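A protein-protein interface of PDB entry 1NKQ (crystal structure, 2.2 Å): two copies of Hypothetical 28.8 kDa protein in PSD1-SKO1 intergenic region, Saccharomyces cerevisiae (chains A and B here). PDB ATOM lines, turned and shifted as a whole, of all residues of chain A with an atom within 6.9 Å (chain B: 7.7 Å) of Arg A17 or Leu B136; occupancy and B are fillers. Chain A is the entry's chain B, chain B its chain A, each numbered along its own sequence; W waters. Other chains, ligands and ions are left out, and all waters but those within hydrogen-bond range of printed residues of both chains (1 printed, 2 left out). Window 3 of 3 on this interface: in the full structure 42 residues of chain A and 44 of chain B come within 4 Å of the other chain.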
ATOM      1  N   ILE A  15      18.503   3.728   7.567  1.00  0.00           N
ATOM      2  CA  ILE A  15      17.081   3.624   7.860  1.00  0.00           C
ATOM      3  C   ILE A  15      16.627   2.220   7.469  1.00  0.00           C
ATOM      4  O   ILE A  15      17.109   1.656   6.489  1.00  0.00           O
ATOM      5  CB  ILE A  15      16.250   4.678   7.079  1.00  0.00           C
ATOM      6  CG1 ILE A  15      14.791   4.628   7.545  1.00  0.00           C
ATOM      7  CG2 ILE A  15      16.329   4.416   5.581  1.00  0.00           C
ATOM      8  CD1 ILE A  15      13.956   5.791   7.080  1.00  0.00           C
ATOM      9  N   GLY A  16      15.715   1.644   8.244  1.00  0.00           N
ATOM     10  CA  GLY A  16      15.245   0.309   7.926  1.00  0.00           C
ATOM     11  C   GLY A  16      13.845   0.277   7.341  1.00  0.00           C
ATOM     12  O   GLY A  16      13.112   1.264   7.404  1.00  0.00           O
ATOM     13  N   ARG A  17      13.493  -0.863   6.752  1.00  0.00           N
ATOM     14  CA  ARG A  17      12.170  -1.090   6.163  1.00  0.00           C
ATOM     15  C   ARG A  17      11.600   0.198   5.567  1.00  0.00           C
ATOM     16  O   ARG A  17      10.608   0.739   6.077  1.00  0.00           O
ATOM     17  CB  ARG A  17      11.236  -1.626   7.250  1.00  0.00           C
ATOM     18  CG  ARG A  17      11.782  -2.865   7.954  1.00  0.00           C
ATOM     19  CD  ARG A  17      11.028  -3.141   9.248  1.00  0.00           C
ATOM     20  NE  ARG A  17      11.607  -4.260   9.989  1.00  0.00           N
ATOM     21  CZ  ARG A  17      11.589  -4.362  11.315  1.00  0.00           C
ATOM     22  NH1 ARG A  17      11.019  -3.410  12.043  1.00  0.00           N
ATOM     23  NH2 ARG A  17      12.153  -5.406  11.913  1.00  0.00           N
ATOM     24  N   ASN A  18      12.209   0.660   4.475  1.00  0.00           N
ATOM     25  CA  ASN A  18      11.816   1.917   3.850  1.00  0.00           C
ATOM     26  C   ASN A  18      11.296   1.803   2.424  1.00  0.00           C
ATOM     27  O   ASN A  18      11.219   2.805   1.719  1.00  0.00           O
ATOM     28  CB  ASN A  18      13.013   2.875   3.873  1.00  0.00           C
ATOM     29  CG  ASN A  18      12.611   4.333   3.710  1.00  0.00           C
ATOM     30  OD1 ASN A  18      13.429   5.173   3.321  1.00  0.00           O
ATOM     31  ND2 ASN A  18      11.358   4.646   4.032  1.00  0.00           N
ATOM     32  N   TYR A  19      10.950   0.596   1.987  1.00  0.00           N
ATOM     33  CA  TYR A  19      10.436   0.420   0.631  1.00  0.00           C
ATOM     34  C   TYR A  19       9.106  -0.323   0.574  1.00  0.00           C
ATOM     35  O   TYR A  19       8.899  -1.310   1.282  1.00  0.00           O
ATOM     36  CB  TYR A  19      11.452  -0.317  -0.237  1.00  0.00           C
ATOM     37  CG  TYR A  19      12.494   0.577  -0.860  1.00  0.00           C
ATOM     38  CD1 TYR A  19      13.520   1.125  -0.096  1.00  0.00           C
ATOM     39  CD2 TYR A  19      12.466   0.854  -2.223  1.00  0.00           C
ATOM     40  CE1 TYR A  19      14.500   1.928  -0.677  1.00  0.00           C
ATOM     41  CE2 TYR A  19      13.438   1.652  -2.814  1.00  0.00           C
ATOM     42  CZ  TYR A  19      14.453   2.181  -2.036  1.00  0.00           C
ATOM     43  OH  TYR A  19      15.436   2.936  -2.620  1.00  0.00           O
ATOM     44  N   ALA A  20       8.207   0.152  -0.279  1.00  0.00           N
ATOM     45  CA  ALA A  20       6.906  -0.476  -0.418  1.00  0.00           C
ATOM     46  C   ALA A  20       7.037  -1.790  -1.174  1.00  0.00           C
ATOM     47  O   ALA A  20       7.681  -1.851  -2.220  1.00  0.00           O
ATOM     48  CB  ALA A  20       5.960   0.453  -1.144  1.00  0.00           C
ATOM     49  N   GLN A  33       7.518   5.193  13.269  1.00  0.00           N
ATOM     50  CA  GLN A  33       7.409   4.157  12.249  1.00  0.00           C
ATOM     51  C   GLN A  33       8.781   3.732  11.716  1.00  0.00           C
ATOM     52  O   GLN A  33       9.034   2.542  11.508  1.00  0.00           O
ATOM     53  CB  GLN A  33       6.516   4.646  11.094  1.00  0.00           C
ATOM     54  N   PRO A  34       9.682   4.697  11.473  1.00  0.00           N
ATOM     55  CA  PRO A  34      10.995   4.305  10.962  1.00  0.00           C
ATOM     56  C   PRO A  34      12.035   4.160  12.067  1.00  0.00           C
ATOM     57  O   PRO A  34      11.995   4.873  13.074  1.00  0.00           O
ATOM     58  CB  PRO A  34      11.337   5.447  10.016  1.00  0.00           C
ATOM     59  CG  PRO A  34      10.832   6.629  10.783  1.00  0.00           C
ATOM     60  CD  PRO A  34       9.474   6.150  11.301  1.00  0.00           C
ATOM     61  N   PHE A  35      12.964   3.232  11.876  1.00  0.00           N
ATOM     62  CA  PHE A  35      14.023   3.034  12.848  1.00  0.00           C
ATOM     63  C   PHE A  35      15.362   3.224  12.140  1.00  0.00           C
ATOM     64  O   PHE A  35      15.442   3.110  10.913  1.00  0.00           O
ATOM     65  CB  PHE A  35      13.903   1.647  13.502  1.00  0.00           C
ATOM     66  CG  PHE A  35      14.026   0.501  12.550  1.00  0.00           C
ATOM     67  CD1 PHE A  35      15.278   0.056  12.136  1.00  0.00           C
ATOM     68  CD2 PHE A  35      12.891  -0.156  12.084  1.00  0.00           C
ATOM     69  CE1 PHE A  35      15.402  -1.022  11.280  1.00  0.00           C
ATOM     70  CE2 PHE A  35      13.005  -1.245  11.220  1.00  0.00           C
ATOM     71  CZ  PHE A  35      14.264  -1.677  10.819  1.00  0.00           C
ATOM     72  N   PHE A  36      16.399   3.542  12.912  1.00  0.00           N
ATOM     73  CA  PHE A  36      17.727   3.774  12.357  1.00  0.00           C
ATOM     74  C   PHE A  36      18.810   3.037  13.123  1.00  0.00           C
ATOM     75  O   PHE A  36      18.666   2.738  14.311  1.00  0.00           O
ATOM     76  CB  PHE A  36      18.063   5.271  12.377  1.00  0.00           C
ATOM     77  CG  PHE A  36      17.003   6.136  11.771  1.00  0.00           C
ATOM     78  CD1 PHE A  36      15.843   6.429  12.477  1.00  0.00           C
ATOM     79  CD2 PHE A  36      17.154   6.645  10.485  1.00  0.00           C
ATOM     80  CE1 PHE A  36      14.845   7.204  11.912  1.00  0.00           C
ATOM     81  CE2 PHE A  36      16.157   7.424   9.908  1.00  0.00           C
ATOM     82  CZ  PHE A  36      15.005   7.707  10.621  1.00  0.00           C
ATOM     83  N   PHE A  37      19.909   2.760  12.437  1.00  0.00           N
ATOM     84  CA  PHE A  37      21.033   2.074  13.050  1.00  0.00           C
ATOM     85  C   PHE A  37      22.313   2.566  12.398  1.00  0.00           C
ATOM     86  O   PHE A  37      22.289   3.039  11.264  1.00  0.00           O
ATOM     87  CB  PHE A  37      20.885   0.558  12.885  1.00  0.00           C
ATOM     88  CG  PHE A  37      20.836   0.104  11.454  1.00  0.00           C
ATOM     89  CD1 PHE A  37      22.011  -0.069  10.724  1.00  0.00           C
ATOM     90  CD2 PHE A  37      19.613  -0.124  10.828  1.00  0.00           C
ATOM     91  CE1 PHE A  37      21.967  -0.465   9.389  1.00  0.00           C
ATOM     92  CE2 PHE A  37      19.556  -0.519   9.493  1.00  0.00           C
ATOM     93  CZ  PHE A  37      20.734  -0.689   8.771  1.00  0.00           C
ATOM     94  N   GLN A 128      21.552 -11.353  13.563  1.00  0.00           N
ATOM     95  CA  GLN A 128      20.547 -10.327  13.829  1.00  0.00           C
ATOM     96  C   GLN A 128      19.268 -10.966  14.370  1.00  0.00           C
ATOM     97  O   GLN A 128      18.581 -10.385  15.217  1.00  0.00           O
ATOM     98  CB  GLN A 128      20.226  -9.537  12.554  1.00  0.00           C
ATOM     99  CG  GLN A 128      19.101  -8.515  12.737  1.00  0.00           C
ATOM    100  CD  GLN A 128      18.572  -7.959  11.422  1.00  0.00           C
ATOM    101  OE1 GLN A 128      18.302  -8.710  10.491  1.00  0.00           O
ATOM    102  NE2 GLN A 128      18.398  -6.644  11.351  1.00  0.00           N
ATOM    103  N   ALA A 131      19.753 -11.364  17.836  1.00  0.00           N
ATOM    104  CA  ALA A 131      19.800 -10.081  18.531  1.00  0.00           C
ATOM    105  C   ALA A 131      18.381  -9.565  18.744  1.00  0.00           C
ATOM    106  O   ALA A 131      18.041  -9.076  19.827  1.00  0.00           O
ATOM    107  CB  ALA A 131      20.621  -9.069  17.735  1.00  0.00           C
ATOM    108  N   LYS A 132      17.554  -9.673  17.710  1.00  0.00           N
ATOM    109  CA  LYS A 132      16.168  -9.232  17.802  1.00  0.00           C
ATOM    110  C   LYS A 132      15.438 -10.043  18.875  1.00  0.00           C
ATOM    111  O   LYS A 132      14.654  -9.499  19.653  1.00  0.00           O
ATOM    112  CB  LYS A 132      15.475  -9.385  16.444  1.00  0.00           C
ATOM    113  CG  LYS A 132      16.129  -8.550  15.354  1.00  0.00           C
ATOM    114  CD  LYS A 132      15.666  -8.934  13.956  1.00  0.00           C
ATOM    115  CE  LYS A 132      14.280  -8.409  13.653  1.00  0.00           C
ATOM    116  NZ  LYS A 132      13.849  -8.780  12.274  1.00  0.00           N
ATOM    117  N   GLY A 135      16.613  -8.871  22.161  1.00  0.00           N
ATOM    118  CA  GLY A 135      16.509  -7.430  22.305  1.00  0.00           C
ATOM    119  C   GLY A 135      17.872  -6.810  22.544  1.00  0.00           C
ATOM    120  O   GLY A 135      18.015  -5.858  23.318  1.00  0.00           O
ATOM    121  N   LEU A 136      18.880  -7.363  21.877  1.00  0.00           N
ATOM    122  CA  LEU A 136      20.245  -6.881  22.004  1.00  0.00           C
ATOM    123  C   LEU A 136      20.641  -6.033  20.790  1.00  0.00           C
ATOM    124  O   LEU A 136      19.968  -6.059  19.760  1.00  0.00           O
ATOM    125  CB  LEU A 136      21.190  -8.073  22.189  1.00  0.00           C
ATOM    126  CG  LEU A 136      20.938  -8.874  23.476  1.00  0.00           C
ATOM    127  CD1 LEU A 136      21.866 -10.075  23.551  1.00  0.00           C
ATOM    128  CD2 LEU A 136      21.143  -7.971  24.681  1.00  0.00           C
ATOM    129  N   PRO A 137      21.734  -5.262  20.901  1.00  0.00           N
ATOM    130  CA  PRO A 137      22.211  -4.401  19.811  1.00  0.00           C
ATOM    131  C   PRO A 137      22.421  -5.116  18.470  1.00  0.00           C
ATOM    132  O   PRO A 137      22.832  -6.275  18.433  1.00  0.00           O
ATOM    133  CB  PRO A 137      23.518  -3.822  20.372  1.00  0.00           C
ATOM    134  CG  PRO A 137      23.286  -3.809  21.835  1.00  0.00           C
ATOM    135  CD  PRO A 137      22.608  -5.138  22.082  1.00  0.00           C
ATOM    136  N   TRP A 138      22.137  -4.400  17.383  1.00  0.00           N
ATOM    137  CA  TRP A 138      22.283  -4.900  16.011  1.00  0.00           C
ATOM    138  C   TRP A 138      23.704  -4.690  15.485  1.00  0.00           C
ATOM    139  O   TRP A 138      24.094  -5.287  14.476  1.00  0.00           O
ATOM    140  CB  TRP A 138      21.333  -4.141  15.076  1.00  0.00           C
ATOM    141  CG  TRP A 138      19.900  -4.545  15.118  1.00  0.00           C
ATOM    142  CD1 TRP A 138      19.233  -5.133  16.156  1.00  0.00           C
ATOM    143  CD2 TRP A 138      18.928  -4.338  14.090  1.00  0.00           C
ATOM    144  NE1 TRP A 138      17.904  -5.299  15.837  1.00  0.00           N
ATOM    145  CE2 TRP A 138      17.691  -4.812  14.572  1.00  0.00           C
ATOM    146  CE3 TRP A 138      18.984  -3.779  12.804  1.00  0.00           C
ATOM    147  CZ2 TRP A 138      16.518  -4.765  13.813  1.00  0.00           C
ATOM    148  CZ3 TRP A 138      17.813  -3.732  12.046  1.00  0.00           C
ATOM    149  CH2 TRP A 138      16.599  -4.217  12.558  1.00  0.00           C
ATOM    150  N   LEU A 190       9.235   4.716   1.217  1.00  0.00           N
ATOM    151  CA  LEU A 190       8.147   5.050   2.133  1.00  0.00           C
ATOM    152  C   LEU A 190       8.389   6.427   2.713  1.00  0.00           C
ATOM    153  O   LEU A 190       7.543   7.315   2.622  1.00  0.00           O
ATOM    154  CB  LEU A 190       8.064   4.004   3.239  1.00  0.00           C
ATOM    155  CG  LEU A 190       7.711   2.615   2.702  1.00  0.00           C
ATOM    156  CD1 LEU A 190       7.839   1.563   3.785  1.00  0.00           C
ATOM    157  CD2 LEU A 190       6.308   2.657   2.148  1.00  0.00           C
ATOM    158  N   HIS A 191       9.556   6.600   3.316  1.00  0.00           N
ATOM    159  CA  HIS A 191       9.930   7.885   3.876  1.00  0.00           C
ATOM    160  C   HIS A 191      10.888   8.496   2.862  1.00  0.00           C
ATOM    161  O   HIS A 191      11.987   7.985   2.645  1.00  0.00           O
ATOM    162  CB  HIS A 191      10.620   7.699   5.225  1.00  0.00           C
ATOM    163  CG  HIS A 191       9.745   7.074   6.262  1.00  0.00           C
ATOM    164  ND1 HIS A 191       9.537   5.713   6.338  1.00  0.00           N
ATOM    165  CD2 HIS A 191       8.989   7.623   7.239  1.00  0.00           C
ATOM    166  CE1 HIS A 191       8.691   5.452   7.317  1.00  0.00           C
ATOM    167  NE2 HIS A 191       8.341   6.595   7.880  1.00  0.00           N
ATOM    168  N   THR A 214      19.613   4.943   2.587  1.00  0.00           N
ATOM    169  CA  THR A 214      18.170   5.133   2.566  1.00  0.00           C
ATOM    170  C   THR A 214      17.210   3.946   2.452  1.00  0.00           C
ATOM    171  O   THR A 214      16.030   4.144   2.177  1.00  0.00           O
ATOM    172  CB  THR A 214      17.823   6.136   1.461  1.00  0.00           C
ATOM    173  OG1 THR A 214      18.138   5.563   0.185  1.00  0.00           O
ATOM    174  CG2 THR A 214      18.643   7.407   1.640  1.00  0.00           C
ATOM    175  N   GLY A 215      17.690   2.725   2.663  1.00  0.00           N
ATOM    176  CA  GLY A 215      16.802   1.579   2.580  1.00  0.00           C
ATOM    177  C   GLY A 215      16.971   0.725   1.339  1.00  0.00           C
ATOM    178  O   GLY A 215      17.504   1.162   0.317  1.00  0.00           O
ATOM    179  N   THR A 216      16.498  -0.510   1.417  1.00  0.00           N
ATOM    180  CA  THR A 216      16.625  -1.423   0.293  1.00  0.00           C
ATOM    181  C   THR A 216      15.264  -1.895  -0.223  1.00  0.00           C
ATOM    182  O   THR A 216      14.291  -1.992   0.532  1.00  0.00           O
ATOM    183  CB  THR A 216      17.469  -2.656   0.700  1.00  0.00           C
ATOM    184  OG1 THR A 216      17.857  -3.387  -0.469  1.00  0.00           O
ATOM    185  CG2 THR A 216      16.669  -3.566   1.630  1.00  0.00           C
ATOM    186  N   VAL B 127      13.330   4.867  25.695  1.00  0.00           N
ATOM    187  CA  VAL B 127      13.436   4.668  24.256  1.00  0.00           C
ATOM    188  C   VAL B 127      14.091   3.299  24.043  1.00  0.00           C
ATOM    189  O   VAL B 127      13.764   2.576  23.093  1.00  0.00           O
ATOM    190  CB  VAL B 127      14.323   5.749  23.595  1.00  0.00           C
ATOM    191  CG1 VAL B 127      14.519   5.438  22.120  1.00  0.00           C
ATOM    192  CG2 VAL B 127      13.700   7.119  23.779  1.00  0.00           C
ATOM    193  N   GLN B 128      15.012   2.943  24.934  1.00  0.00           N
ATOM    194  CA  GLN B 128      15.697   1.661  24.830  1.00  0.00           C
ATOM    195  C   GLN B 128      14.792   0.509  25.265  1.00  0.00           C
ATOM    196  O   GLN B 128      14.864  -0.582  24.704  1.00  0.00           O
ATOM    197  CB  GLN B 128      16.975   1.656  25.670  1.00  0.00           C
ATOM    198  CG  GLN B 128      17.744   0.340  25.601  1.00  0.00           C
ATOM    199  CD  GLN B 128      18.847   0.260  26.643  1.00  0.00           C
ATOM    200  OE1 GLN B 128      18.674   0.704  27.778  1.00  0.00           O
ATOM    201  NE2 GLN B 128      19.983  -0.321  26.267  1.00  0.00           N
ATOM    202  N   GLU B 130      11.645   0.274  24.832  1.00  0.00           N
ATOM    203  CA  GLU B 130      10.786   0.049  23.676  1.00  0.00           C
ATOM    204  C   GLU B 130      11.509  -0.719  22.565  1.00  0.00           C
ATOM    205  O   GLU B 130      10.941  -1.628  21.969  1.00  0.00           O
ATOM    206  CB  GLU B 130      10.263   1.387  23.137  1.00  0.00           C
ATOM    207  CG  GLU B 130       9.387   1.251  21.895  1.00  0.00           C
ATOM    208  CD  GLU B 130       8.798   2.573  21.430  1.00  0.00           C
ATOM    209  OE1 GLU B 130       7.872   3.092  22.093  1.00  0.00           O
ATOM    210  OE2 GLU B 130       9.267   3.101  20.400  1.00  0.00           O
ATOM    211  N   ALA B 131      12.757  -0.350  22.291  1.00  0.00           N
ATOM    212  CA  ALA B 131      13.540  -1.012  21.257  1.00  0.00           C
ATOM    213  C   ALA B 131      13.717  -2.477  21.616  1.00  0.00           C
ATOM    214  O   ALA B 131      13.579  -3.350  20.764  1.00  0.00           O
ATOM    215  CB  ALA B 131      14.905  -0.348  21.110  1.00  0.00           C
ATOM    216  N   LYS B 132      14.031  -2.737  22.884  1.00  0.00           N
ATOM    217  CA  LYS B 132      14.218  -4.102  23.369  1.00  0.00           C
ATOM    218  C   LYS B 132      12.980  -4.931  23.079  1.00  0.00           C
ATOM    219  O   LYS B 132      13.065  -6.002  22.486  1.00  0.00           O
ATOM    220  CB  LYS B 132      14.479  -4.122  24.884  1.00  0.00           C
ATOM    221  CG  LYS B 132      15.865  -3.669  25.317  1.00  0.00           C
ATOM    222  CD  LYS B 132      16.020  -3.762  26.831  1.00  0.00           C
ATOM    223  CE  LYS B 132      17.393  -3.309  27.293  1.00  0.00           C
ATOM    224  NZ  LYS B 132      17.453  -3.142  28.784  1.00  0.00           N
ATOM    225  N   LYS B 133      11.826  -4.428  23.503  1.00  0.00           N
ATOM    226  CA  LYS B 133      10.573  -5.140  23.296  1.00  0.00           C
ATOM    227  C   LYS B 133      10.311  -5.435  21.825  1.00  0.00           C
ATOM    228  O   LYS B 133       9.957  -6.557  21.464  1.00  0.00           O
ATOM    229  CB  LYS B 133       9.406  -4.340  23.887  1.00  0.00           C
ATOM    230  CG  LYS B 133       9.497  -4.186  25.398  1.00  0.00           C
ATOM    231  CD  LYS B 133       8.228  -3.606  26.016  1.00  0.00           C
ATOM    232  CE  LYS B 133       8.374  -3.478  27.540  1.00  0.00           C
ATOM    233  NZ  LYS B 133       7.093  -3.090  28.203  1.00  0.00           N
ATOM    234  N   LYS B 134      10.500  -4.427  20.980  1.00  0.00           N
ATOM    235  CA  LYS B 134      10.276  -4.570  19.551  1.00  0.00           C
ATOM    236  C   LYS B 134      11.439  -5.229  18.812  1.00  0.00           C
ATOM    237  O   LYS B 134      11.358  -5.466  17.609  1.00  0.00           O
ATOM    238  CB  LYS B 134       9.990  -3.200  18.939  1.00  0.00           C
ATOM    239  CG  LYS B 134       8.791  -2.492  19.559  1.00  0.00           C
ATOM    240  CD  LYS B 134       8.500  -1.174  18.855  1.00  0.00           C
ATOM    241  CE  LYS B 134       7.321  -0.455  19.502  1.00  0.00           C
ATOM    242  NZ  LYS B 134       6.985   0.829  18.815  1.00  0.00           N
ATOM    243  N   GLY B 135      12.512  -5.533  19.534  1.00  0.00           N
ATOM    244  CA  GLY B 135      13.669  -6.155  18.916  1.00  0.00           C
ATOM    245  C   GLY B 135      14.297  -5.253  17.868  1.00  0.00           C
ATOM    246  O   GLY B 135      14.758  -5.721  16.833  1.00  0.00           O
ATOM    247  N   LEU B 136      14.316  -3.951  18.141  1.00  0.00           N
ATOM    248  CA  LEU B 136      14.889  -2.984  17.215  1.00  0.00           C
ATOM    249  C   LEU B 136      16.226  -2.415  17.707  1.00  0.00           C
ATOM    250  O   LEU B 136      16.593  -2.572  18.870  1.00  0.00           O
ATOM    251  CB  LEU B 136      13.873  -1.870  16.963  1.00  0.00           C
ATOM    252  CG  LEU B 136      12.657  -2.367  16.168  1.00  0.00           C
ATOM    253  CD1 LEU B 136      11.596  -1.282  16.071  1.00  0.00           C
ATOM    254  CD2 LEU B 136      13.111  -2.800  14.773  1.00  0.00           C
ATOM    255  N   PRO B 137      16.978  -1.752  16.817  1.00  0.00           N
ATOM    256  CA  PRO B 137      18.277  -1.168  17.173  1.00  0.00           C
ATOM    257  C   PRO B 137      18.284  -0.167  18.333  1.00  0.00           C
ATOM    258  O   PRO B 137      17.315   0.551  18.562  1.00  0.00           O
ATOM    259  CB  PRO B 137      18.748  -0.547  15.856  1.00  0.00           C
ATOM    260  CG  PRO B 137      17.482  -0.246  15.141  1.00  0.00           C
ATOM    261  CD  PRO B 137      16.658  -1.477  15.406  1.00  0.00           C
ATOM    262  N   TRP B 138      19.406  -0.137  19.051  1.00  0.00           N
ATOM    263  CA  TRP B 138      19.619   0.744  20.204  1.00  0.00           C
ATOM    264  C   TRP B 138      20.224   2.087  19.791  1.00  0.00           C
ATOM    265  O   TRP B 138      20.345   2.991  20.619  1.00  0.00           O
ATOM    266  CB  TRP B 138      20.613   0.113  21.178  1.00  0.00           C
ATOM    267  CG  TRP B 138      20.186  -1.124  21.880  1.00  0.00           C
ATOM    268  CD1 TRP B 138      19.189  -1.991  21.518  1.00  0.00           C
ATOM    269  CD2 TRP B 138      20.768  -1.660  23.070  1.00  0.00           C
ATOM    270  NE1 TRP B 138      19.114  -3.030  22.418  1.00  0.00           N
ATOM    271  CE2 TRP B 138      20.075  -2.846  23.385  1.00  0.00           C
ATOM    272  CE3 TRP B 138      21.818  -1.238  23.909  1.00  0.00           C
ATOM    273  CZ2 TRP B 138      20.390  -3.628  24.502  1.00  0.00           C
ATOM    274  CZ3 TRP B 138      22.135  -2.017  25.022  1.00  0.00           C
ATOM    275  CH2 TRP B 138      21.419  -3.196  25.308  1.00  0.00           C
ATOM    276  N   THR B 139      20.617   2.198  18.523  1.00  0.00           N
ATOM    277  CA  THR B 139      21.262   3.405  18.004  1.00  0.00           C
ATOM    278  C   THR B 139      20.745   4.738  18.532  1.00  0.00           C
ATOM    279  O   THR B 139      21.508   5.505  19.119  1.00  0.00           O
ATOM    280  CB  THR B 139      21.240   3.437  16.458  1.00  0.00           C
ATOM    281  OG1 THR B 139      22.163   2.465  15.951  1.00  0.00           O
ATOM    282  CG2 THR B 139      21.651   4.807  15.944  1.00  0.00           C
ATOM    283  N   SER B 141      18.640   5.413  21.080  1.00  0.00           N
ATOM    284  CA  SER B 141      18.695   5.495  22.537  1.00  0.00           C
ATOM    285  C   SER B 141      20.108   5.673  23.077  1.00  0.00           C
ATOM    286  O   SER B 141      20.292   6.031  24.242  1.00  0.00           O
ATOM    287  CB  SER B 141      18.093   4.247  23.170  1.00  0.00           C
ATOM    288  OG  SER B 141      19.020   3.175  23.133  1.00  0.00           O
HETATM  289  O   HOH W   1      17.888   2.825  16.968  1.00  0.00           O
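The indole nitrogen of Trp A138 is in hydrogen-bond range of the backbone carbonyl oxygen of Gly B135 (3.3 Å).
The backbone carbonyl oxygen of Gly A135 sits at hydrogen-bond distance from the indole nitrogen of Trp B138 (3.2 Å).
The backbone carbonyl oxygen (O) of Ala B131 is in hydrogen-bond range of the backbone NH (N) of Leu B136 (2.8 Å).
The side-chain hydroxyl (OG) of Ser B141 sits at hydrogen-bond distance from the backbone carbonyl oxygen (O) of Trp B138, 2.8 Å away.
N of Gly A16 sits at hydrogen-bond distance from O of Phe A35, 3.1 Å away.
The backbone carbonyl oxygen (O) of Ala A131 sits at hydrogen-bond distance from the backbone NH (N) of Leu A136 (2.8 Å).
Arg A17 touches Leu B136.
CD2 of Phe A35 touches CD2 of Leu B136, at 3.8 Å.
Phe A35 touches Pro B137 (CD1 to CG, 3.7 Å).
O of Phe A36 touches CB of Thr B139, at 3.4 Å.
Pro B137 touches Phe A37.
Gly B135 touches Lys A132.
Leu A136 touches Trp B138 (C to NE1, 3.7 Å).
Pro A137 touches Trp B138.
Trp A138 touches Leu B136 (NE1 to C, 3.8 Å).
Trp A138 touches Pro B137.
Of the printed residues of chain B, Arg A17 touches Leu B136.
Of chain A, only Arg A17 (3.5 Å), Phe A35 (3.8 Å) and Trp A138 (3.8 Å) come within 4 Å of Leu B136.
Printed residues of chain B within 4 Å of Gly A135: Lys B132 (3.7 Å) and Trp B138 (3.2 Å).
Of the printed residues of chain A, Pro B137 touches Phe A35, Phe A36, Phe A37 and Trp A138.
Printed residues of chain A within 4 Å of Thr B139: Phe A36 and Phe A37.
Printed residues of chain B within 4 Å of Phe A35: Leu B136 and Pro B137.
Of the printed residues of chain B, Trp A138 touches Gly B135 (3.3 Å), Leu B136 (3.8 Å) and Pro B137 (3.6 Å).
Gln A128 touches none of the printed residues of chain B.
Gly A215 touches none of the printed residues of chain B.
The nearest residue of chain B that does not touch Arg A17 is Gly B135 (5.6 Å).
The nearest residue of chain A that does not touch Leu B136 is Leu A136 (4.9 Å).
The nearest printed residue of chain B that does not touch Phe A35 is Gly B135 (7.3 Å).
Of the 13 printed residues of chain B, 6 touch a printed residue of chain A.
Along chain B the printed residues that touch a printed residue of chain A span positions 132 to 139.
Hydrophobic or aromatic side chains of chain A within 4 Å of the printed part of chain B: Phe A35, Phe A37, Pro A137 and Trp A138.
Lys A132 touches Gly B135, and with the chains exchanged Gly A135 touches Lys B132.
Gly A135 touches Trp B138, and with the chains exchanged Trp A138 touches Gly B135.
Leu A136 touches Trp B138, and with the chains exchanged Trp A138 touches Leu B136.
Pro A137 touches Trp B138, and with the chains exchanged Trp A138 touches Pro B137.
7 positions are printed for both chains.
Water W1 lies within hydrogen-bond range of O of Phe A36 (2.8 Å), O of Pro B137 (2.8 Å) and N of Thr B139 (3.2 Å).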
